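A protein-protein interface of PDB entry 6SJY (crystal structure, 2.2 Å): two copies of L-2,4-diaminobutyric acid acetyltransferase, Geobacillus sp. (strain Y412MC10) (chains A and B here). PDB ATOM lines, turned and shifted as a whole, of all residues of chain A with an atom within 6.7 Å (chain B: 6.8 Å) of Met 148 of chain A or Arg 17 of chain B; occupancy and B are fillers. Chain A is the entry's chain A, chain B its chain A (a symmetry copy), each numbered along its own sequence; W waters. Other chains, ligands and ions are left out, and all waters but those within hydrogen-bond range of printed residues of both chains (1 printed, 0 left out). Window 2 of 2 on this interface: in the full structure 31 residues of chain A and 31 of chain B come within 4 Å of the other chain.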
ATOM      1  N   GLY A 143     -17.321  17.695 -23.115  1.00  0.00           N
ATOM      2  CA  GLY A 143     -16.191  16.761 -23.112  1.00  0.00           C
ATOM      3  C   GLY A 143     -15.084  17.404 -22.314  1.00  0.00           C
ATOM      4  O   GLY A 143     -15.225  17.500 -21.149  1.00  0.00           O
ATOM      5  N   TYR A 144     -14.017  17.890 -22.941  1.00  0.00           N
ATOM      6  CA  TYR A 144     -12.988  18.667 -22.238  1.00  0.00           C
ATOM      7  C   TYR A 144     -13.318  20.112 -22.590  1.00  0.00           C
ATOM      8  O   TYR A 144     -13.501  20.451 -23.783  1.00  0.00           O
ATOM      9  CB  TYR A 144     -11.543  18.330 -22.748  1.00  0.00           C
ATOM     10  CG  TYR A 144     -11.199  16.846 -22.717  1.00  0.00           C
ATOM     11  CD1 TYR A 144     -11.439  16.081 -21.554  1.00  0.00           C
ATOM     12  CD2 TYR A 144     -10.595  16.223 -23.791  1.00  0.00           C
ATOM     13  CE1 TYR A 144     -11.146  14.722 -21.500  1.00  0.00           C
ATOM     14  CE2 TYR A 144     -10.292  14.833 -23.753  1.00  0.00           C
ATOM     15  CZ  TYR A 144     -10.557  14.110 -22.598  1.00  0.00           C
ATOM     16  OH  TYR A 144     -10.332  12.775 -22.531  1.00  0.00           O
ATOM     17  N   GLY A 145     -13.258  20.973 -21.600  1.00  0.00           N
ATOM     18  CA  GLY A 145     -13.415  22.447 -21.803  1.00  0.00           C
ATOM     19  C   GLY A 145     -12.099  23.045 -22.250  1.00  0.00           C
ATOM     20  O   GLY A 145     -11.016  22.490 -21.947  1.00  0.00           O
ATOM     21  N   ALA A 146     -12.179  24.188 -22.919  1.00  0.00           N
ATOM     22  CA  ALA A 146     -11.028  24.972 -23.312  1.00  0.00           C
ATOM     23  C   ALA A 146     -10.080  25.291 -22.181  1.00  0.00           C
ATOM     24  O   ALA A 146      -8.869  25.314 -22.359  1.00  0.00           O
ATOM     25  CB  ALA A 146     -11.490  26.250 -23.963  1.00  0.00           C
ATOM     26  N   GLU A 147     -10.640  25.518 -21.011  1.00  0.00           N
ATOM     27  CA  GLU A 147      -9.873  25.897 -19.879  1.00  0.00           C
ATOM     28  C   GLU A 147      -8.987  24.768 -19.347  1.00  0.00           C
ATOM     29  O   GLU A 147      -8.165  25.020 -18.525  1.00  0.00           O
ATOM     30  CB  GLU A 147     -10.785  26.419 -18.758  1.00  0.00           C
ATOM     31  CG  GLU A 147     -11.673  25.369 -18.099  1.00  0.00           C
ATOM     32  CD  GLU A 147     -12.940  24.998 -18.906  1.00  0.00           C
ATOM     33  OE1 GLU A 147     -13.238  25.559 -20.015  1.00  0.00           O
ATOM     34  OE2 GLU A 147     -13.661  24.115 -18.413  1.00  0.00           O
ATOM     35  N   MET A 148      -9.166  23.528 -19.773  1.00  0.00           N
ATOM     36  CA  MET A 148      -8.269  22.446 -19.321  1.00  0.00           C
ATOM     37  C   MET A 148      -6.885  22.507 -19.987  1.00  0.00           C
ATOM     38  O   MET A 148      -5.994  21.868 -19.501  1.00  0.00           O
ATOM     39  CB  MET A 148      -8.875  21.081 -19.591  1.00  0.00           C
ATOM     40  CG  MET A 148     -10.012  20.720 -18.670  1.00  0.00           C
ATOM     41  SD  MET A 148     -10.854  19.216 -19.234  1.00  0.00           S
ATOM     42  CE  MET A 148      -9.579  17.989 -18.849  1.00  0.00           C
ATOM     43  N   PHE A 149      -6.765  23.252 -21.086  1.00  0.00           N
ATOM     44  CA  PHE A 149      -5.618  23.304 -21.929  1.00  0.00           C
ATOM     45  C   PHE A 149      -4.621  24.327 -21.386  1.00  0.00           C
ATOM     46  O   PHE A 149      -4.977  25.070 -20.488  1.00  0.00           O
ATOM     47  CB  PHE A 149      -6.009  23.590 -23.357  1.00  0.00           C
ATOM     48  CG  PHE A 149      -6.684  22.427 -23.998  1.00  0.00           C
ATOM     49  CD1 PHE A 149      -8.024  22.195 -23.788  1.00  0.00           C
ATOM     50  CD2 PHE A 149      -5.944  21.483 -24.737  1.00  0.00           C
ATOM     51  CE1 PHE A 149      -8.657  21.066 -24.326  1.00  0.00           C
ATOM     52  CE2 PHE A 149      -6.553  20.330 -25.261  1.00  0.00           C
ATOM     53  CZ  PHE A 149      -7.928  20.127 -25.061  1.00  0.00           C
ATOM     54  N   PRO A 150      -3.371  24.237 -21.798  1.00  0.00           N
ATOM     55  CA  PRO A 150      -2.315  25.063 -21.238  1.00  0.00           C
ATOM     56  C   PRO A 150      -2.506  26.530 -21.441  1.00  0.00           C
ATOM     57  O   PRO A 150      -3.025  26.964 -22.436  1.00  0.00           O
ATOM     58  CB  PRO A 150      -1.070  24.541 -21.927  1.00  0.00           C
ATOM     59  CG  PRO A 150      -1.421  23.161 -22.289  1.00  0.00           C
ATOM     60  CD  PRO A 150      -2.824  23.267 -22.741  1.00  0.00           C
ATOM     61  N   ARG B  12      -0.190   8.744  -7.339  1.00  0.00           N
ATOM     62  CA  ARG B  12      -1.573   8.368  -7.675  1.00  0.00           C
ATOM     63  C   ARG B  12      -1.782   8.178  -9.191  1.00  0.00           C
ATOM     64  O   ARG B  12      -0.966   8.623 -10.007  1.00  0.00           O
ATOM     65  CB  ARG B  12      -2.544   9.462  -7.168  1.00  0.00           C
ATOM     66  CG  ARG B  12      -2.314  10.792  -7.814  1.00  0.00           C
ATOM     67  CD  ARG B  12      -3.299  11.849  -7.351  1.00  0.00           C
ATOM     68  NE  ARG B  12      -2.997  13.166  -7.949  1.00  0.00           N
ATOM     69  CZ  ARG B  12      -3.479  13.599  -9.131  1.00  0.00           C
ATOM     70  NH1 ARG B  12      -4.247  12.832  -9.905  1.00  0.00           N
ATOM     71  NH2 ARG B  12      -3.144  14.792  -9.593  1.00  0.00           N
ATOM     72  N   ARG B  13      -2.910   7.590  -9.538  1.00  0.00           N
ATOM     73  CA  ARG B  13      -3.369   7.568 -10.918  1.00  0.00           C
ATOM     74  C   ARG B  13      -3.726   8.960 -11.395  1.00  0.00           C
ATOM     75  O   ARG B  13      -4.211   9.751 -10.633  1.00  0.00           O
ATOM     76  CB  ARG B  13      -4.514   6.604 -11.062  1.00  0.00           C
ATOM     77  CG  ARG B  13      -4.036   5.186 -10.842  1.00  0.00           C
ATOM     78  CD  ARG B  13      -5.069   4.192 -11.308  1.00  0.00           C
ATOM     79  NE  ARG B  13      -6.343   4.396 -10.643  1.00  0.00           N
ATOM     80  CZ  ARG B  13      -6.638   3.962  -9.426  1.00  0.00           C
ATOM     81  NH1 ARG B  13      -5.748   3.301  -8.676  1.00  0.00           N
ATOM     82  NH2 ARG B  13      -7.845   4.222  -8.939  1.00  0.00           N
ATOM     83  N   PRO B  14      -3.350   9.325 -12.635  1.00  0.00           N
ATOM     84  CA  PRO B  14      -3.740  10.653 -13.100  1.00  0.00           C
ATOM     85  C   PRO B  14      -5.214  10.635 -13.459  1.00  0.00           C
ATOM     86  O   PRO B  14      -5.845   9.546 -13.504  1.00  0.00           O
ATOM     87  CB  PRO B  14      -2.912  10.842 -14.388  1.00  0.00           C
ATOM     88  CG  PRO B  14      -2.805   9.434 -14.942  1.00  0.00           C
ATOM     89  CD  PRO B  14      -2.637   8.563 -13.690  1.00  0.00           C
ATOM     90  N   GLU B  15      -5.728  11.816 -13.756  1.00  0.00           N
ATOM     91  CA  GLU B  15      -7.088  12.003 -14.276  1.00  0.00           C
ATOM     92  C   GLU B  15      -6.952  12.935 -15.461  1.00  0.00           C
ATOM     93  O   GLU B  15      -5.896  13.508 -15.658  1.00  0.00           O
ATOM     94  CB  GLU B  15      -7.997  12.602 -13.202  1.00  0.00           C
ATOM     95  CG  GLU B  15      -8.184  11.645 -11.989  1.00  0.00           C
ATOM     96  CD  GLU B  15      -8.827  10.227 -12.290  1.00  0.00           C
ATOM     97  OE1 GLU B  15      -9.974  10.153 -12.823  1.00  0.00           O
ATOM     98  OE2 GLU B  15      -8.223   9.131 -11.970  1.00  0.00           O
ATOM     99  N   ALA B  16      -8.013  13.088 -16.251  1.00  0.00           N
ATOM    100  CA  ALA B  16      -7.961  13.892 -17.443  1.00  0.00           C
ATOM    101  C   ALA B  16      -7.507  15.283 -17.128  1.00  0.00           C
ATOM    102  O   ALA B  16      -6.785  15.919 -17.934  1.00  0.00           O
ATOM    103  CB  ALA B  16      -9.317  13.948 -18.125  1.00  0.00           C
ATOM    104  N   ARG B  17      -7.946  15.799 -15.981  1.00  0.00           N
ATOM    105  CA  ARG B  17      -7.692  17.217 -15.667  1.00  0.00           C
ATOM    106  C   ARG B  17      -6.195  17.404 -15.334  1.00  0.00           C
ATOM    107  O   ARG B  17      -5.708  18.494 -15.415  1.00  0.00           O
ATOM    108  CB  ARG B  17      -8.628  17.701 -14.548  1.00  0.00           C
ATOM    109  CG  ARG B  17      -8.081  17.412 -13.162  1.00  0.00           C
ATOM    110  CD  ARG B  17      -9.073  17.581 -12.011  1.00  0.00           C
ATOM    111  NE  ARG B  17      -9.910  16.389 -11.784  1.00  0.00           N
ATOM    112  CZ  ARG B  17      -9.505  15.207 -11.297  1.00  0.00           C
ATOM    113  NH1 ARG B  17     -10.397  14.228 -11.156  1.00  0.00           N
ATOM    114  NH2 ARG B  17      -8.232  14.984 -10.958  1.00  0.00           N
ATOM    115  N   ASP B  18      -5.450  16.334 -15.024  1.00  0.00           N
ATOM    116  CA  ASP B  18      -3.958  16.440 -14.932  1.00  0.00           C
ATOM    117  C   ASP B  18      -3.216  16.660 -16.239  1.00  0.00           C
ATOM    118  O   ASP B  18      -2.023  16.964 -16.205  1.00  0.00           O
ATOM    119  CB  ASP B  18      -3.384  15.208 -14.266  1.00  0.00           C
ATOM    120  CG  ASP B  18      -3.911  15.023 -12.877  1.00  0.00           C
ATOM    121  OD1 ASP B  18      -3.896  16.030 -12.212  1.00  0.00           O
ATOM    122  OD2 ASP B  18      -4.353  13.911 -12.444  1.00  0.00           O
ATOM    123  N   GLY B  19      -3.899  16.549 -17.380  1.00  0.00           N
ATOM    124  CA  GLY B  19      -3.236  16.424 -18.652  1.00  0.00           C
ATOM    125  C   GLY B  19      -2.254  17.551 -18.852  1.00  0.00           C
ATOM    126  O   GLY B  19      -1.124  17.315 -19.213  1.00  0.00           O
ATOM    127  N   THR B  20      -2.679  18.783 -18.609  1.00  0.00           N
ATOM    128  CA  THR B  20      -1.835  19.947 -18.839  1.00  0.00           C
ATOM    129  C   THR B  20      -0.601  19.986 -17.899  1.00  0.00           C
ATOM    130  O   THR B  20       0.481  20.394 -18.289  1.00  0.00           O
ATOM    131  CB  THR B  20      -2.664  21.246 -18.666  1.00  0.00           C
ATOM    132  OG1 THR B  20      -3.374  21.448 -19.861  1.00  0.00           O
ATOM    133  CG2 THR B  20      -1.781  22.533 -18.459  1.00  0.00           C
ATOM    134  N   ARG B  21      -0.789  19.614 -16.655  1.00  0.00           N
ATOM    135  CA  ARG B  21       0.320  19.641 -15.734  1.00  0.00           C
ATOM    136  C   ARG B  21       1.309  18.538 -16.132  1.00  0.00           C
ATOM    137  O   ARG B  21       2.502  18.737 -16.014  1.00  0.00           O
ATOM    138  CB  ARG B  21      -0.157  19.524 -14.280  1.00  0.00           C
ATOM    139  CG  ARG B  21      -0.288  20.912 -13.614  1.00  0.00           C
ATOM    140  CD  ARG B  21      -1.315  20.936 -12.484  1.00  0.00           C
ATOM    141  NE  ARG B  21      -1.209  19.859 -11.479  1.00  0.00           N
ATOM    142  CZ  ARG B  21      -0.386  19.850 -10.411  1.00  0.00           C
ATOM    143  NH1 ARG B  21       0.482  20.854 -10.161  1.00  0.00           N
ATOM    144  NH2 ARG B  21      -0.425  18.805  -9.564  1.00  0.00           N
ATOM    145  N   VAL B  22       0.804  17.404 -16.637  1.00  0.00           N
ATOM    146  CA  VAL B  22       1.698  16.373 -17.143  1.00  0.00           C
ATOM    147  C   VAL B  22       2.415  16.887 -18.362  1.00  0.00           C
ATOM    148  O   VAL B  22       3.628  16.784 -18.477  1.00  0.00           O
ATOM    149  CB  VAL B  22       0.974  15.065 -17.413  1.00  0.00           C
ATOM    150  CG1 VAL B  22       1.842  14.058 -18.139  1.00  0.00           C
ATOM    151  CG2 VAL B  22       0.462  14.503 -16.077  1.00  0.00           C
ATOM    152  N   PRO B  37      -1.065  18.259 -25.425  1.00  0.00           N
ATOM    153  CA  PRO B  37      -1.786  18.262 -24.152  1.00  0.00           C
ATOM    154  C   PRO B  37      -2.993  17.308 -24.169  1.00  0.00           C
ATOM    155  O   PRO B  37      -3.268  16.591 -23.210  1.00  0.00           O
ATOM    156  CB  PRO B  37      -2.176  19.728 -23.972  1.00  0.00           C
ATOM    157  CG  PRO B  37      -1.192  20.500 -24.790  1.00  0.00           C
ATOM    158  CD  PRO B  37      -0.849  19.598 -25.961  1.00  0.00           C
ATOM    159  N   MET B  41      -4.279  14.275 -21.647  1.00  0.00           N
ATOM    160  CA  MET B  41      -5.634  14.193 -21.082  1.00  0.00           C
ATOM    161  C   MET B  41      -6.262  12.866 -21.360  1.00  0.00           C
ATOM    162  O   MET B  41      -6.894  12.275 -20.460  1.00  0.00           O
ATOM    163  CB  MET B  41      -6.538  15.288 -21.658  1.00  0.00           C
ATOM    164  CG  MET B  41      -6.199  16.701 -21.265  1.00  0.00           C
ATOM    165  SD  MET B  41      -7.158  17.921 -22.248  1.00  0.00           S
ATOM    166  CE  MET B  41      -6.129  19.358 -21.963  1.00  0.00           C
ATOM    167  N   GLY B  44      -4.841  10.393 -18.981  1.00  0.00           N
ATOM    168  CA  GLY B  44      -5.551  10.543 -17.691  1.00  0.00           C
ATOM    169  C   GLY B  44      -6.982   9.996 -17.725  1.00  0.00           C
ATOM    170  O   GLY B  44      -7.510   9.512 -16.745  1.00  0.00           O
ATOM    171  N   ASP B  45      -7.597  10.004 -18.891  1.00  0.00           N
ATOM    172  CA  ASP B  45      -9.010   9.650 -19.014  1.00  0.00           C
ATOM    173  C   ASP B  45      -9.184   8.164 -19.236  1.00  0.00           C
ATOM    174  O   ASP B  45      -9.954   7.529 -18.508  1.00  0.00           O
ATOM    175  CB  ASP B  45      -9.605  10.456 -20.189  1.00  0.00           C
ATOM    176  CG  ASP B  45     -11.136  10.730 -20.056  1.00  0.00           C
ATOM    177  OD1 ASP B  45     -11.782  10.175 -19.183  1.00  0.00           O
ATOM    178  OD2 ASP B  45     -11.667  11.530 -20.873  1.00  0.00           O
HETATM  179  O   HOH W   1      -5.600  19.259 -18.029  1.00  0.00           O
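Met 148 of chain A touches four residues of chain B.
Arg 17 of chain B touches just one residue of chain A: Met 148 (3.8 Å).
Of the printed residues of chain A, Thr 20 of chain B touches Met 148 (2.7 Å), Phe 149 (3.5 Å) and Pro 150 (3.4 Å).
Of the printed residues of chain B, Pro 150 of chain A touches Thr 20 (3.4 Å) and Pro 37 (3.7 Å).
Of the printed residues of chain B, Tyr 144 of chain A touches Ala 16 and Asp 45.
The nearest residue of chain B that does not touch Met 148 of chain A is Gly 19 of chain B (5.7 Å).
The nearest printed residue of chain A that does not touch Thr 20 of chain B is Glu 147 of chain A (6.1 Å).
No position is printed for both chains.
Of the 10 pairs that touch across the chains among the printed residues, none has its exchanged pair printed and touching as well.
The side-chain carboxylate of Asp 45 of chain B lies within hydrogen-bond range of the side-chain hydroxyl of Tyr 144 of chain A (2.5 Å).
The backbone carbonyl oxygen (O) of Met 148 of chain A lies within hydrogen-bond range of the side-chain hydroxyl (OG1) of Thr 20 of chain B (2.7 Å).
The backbone nitrogen of Pro 150 of chain A sits close to the side-chain hydroxyl of Thr 20 of chain B.
Of the 8 printed residues of chain A, 4 touch a printed residue of chain B.
Hydrophobic or aromatic side chains of chain A within 4 Å of the printed part of chain B: Tyr 144, Met 148, Phe 149 and Pro 150.
Of the 15 printed residues of chain B, 6 touch a printed residue of chain A.
Among the printed residues, no Asp or Glu carboxylate lies within 4 Å of a Lys or Arg side-chain nitrogen of the other chain.
Water W1 lies within hydrogen-bond range of the backbone carbonyl oxygen (O) of Arg 17 of chain B (2.7 Å), the backbone NH (N) of Thr 20 of chain B (3.0 Å), the backbone carbonyl oxygen (O) of Met 148 of chain A (3.0 Å) and the backbone NH (N) of Gly 19 of chain B (3.3 Å).
Ala 16 of chain B touches Tyr 144 of chain A.
O of Ala 16 of chain B touches CE of Met 148 of chain A (3.6 Å).
Met 148 of chain A touches Arg 17 of chain B.
Met 148 of chain A touches Met 41 of chain B.
Thr 20 of chain B touches Phe 149 of chain A (OG1 to C, 3.5 Å).
Phe 149 of chain A touches Met 41 of chain B (CE2 to CE, 3.5 Å).
CG of Pro 37 of chain B touches CG of Pro 150 of chain A, 3.7 Å away.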
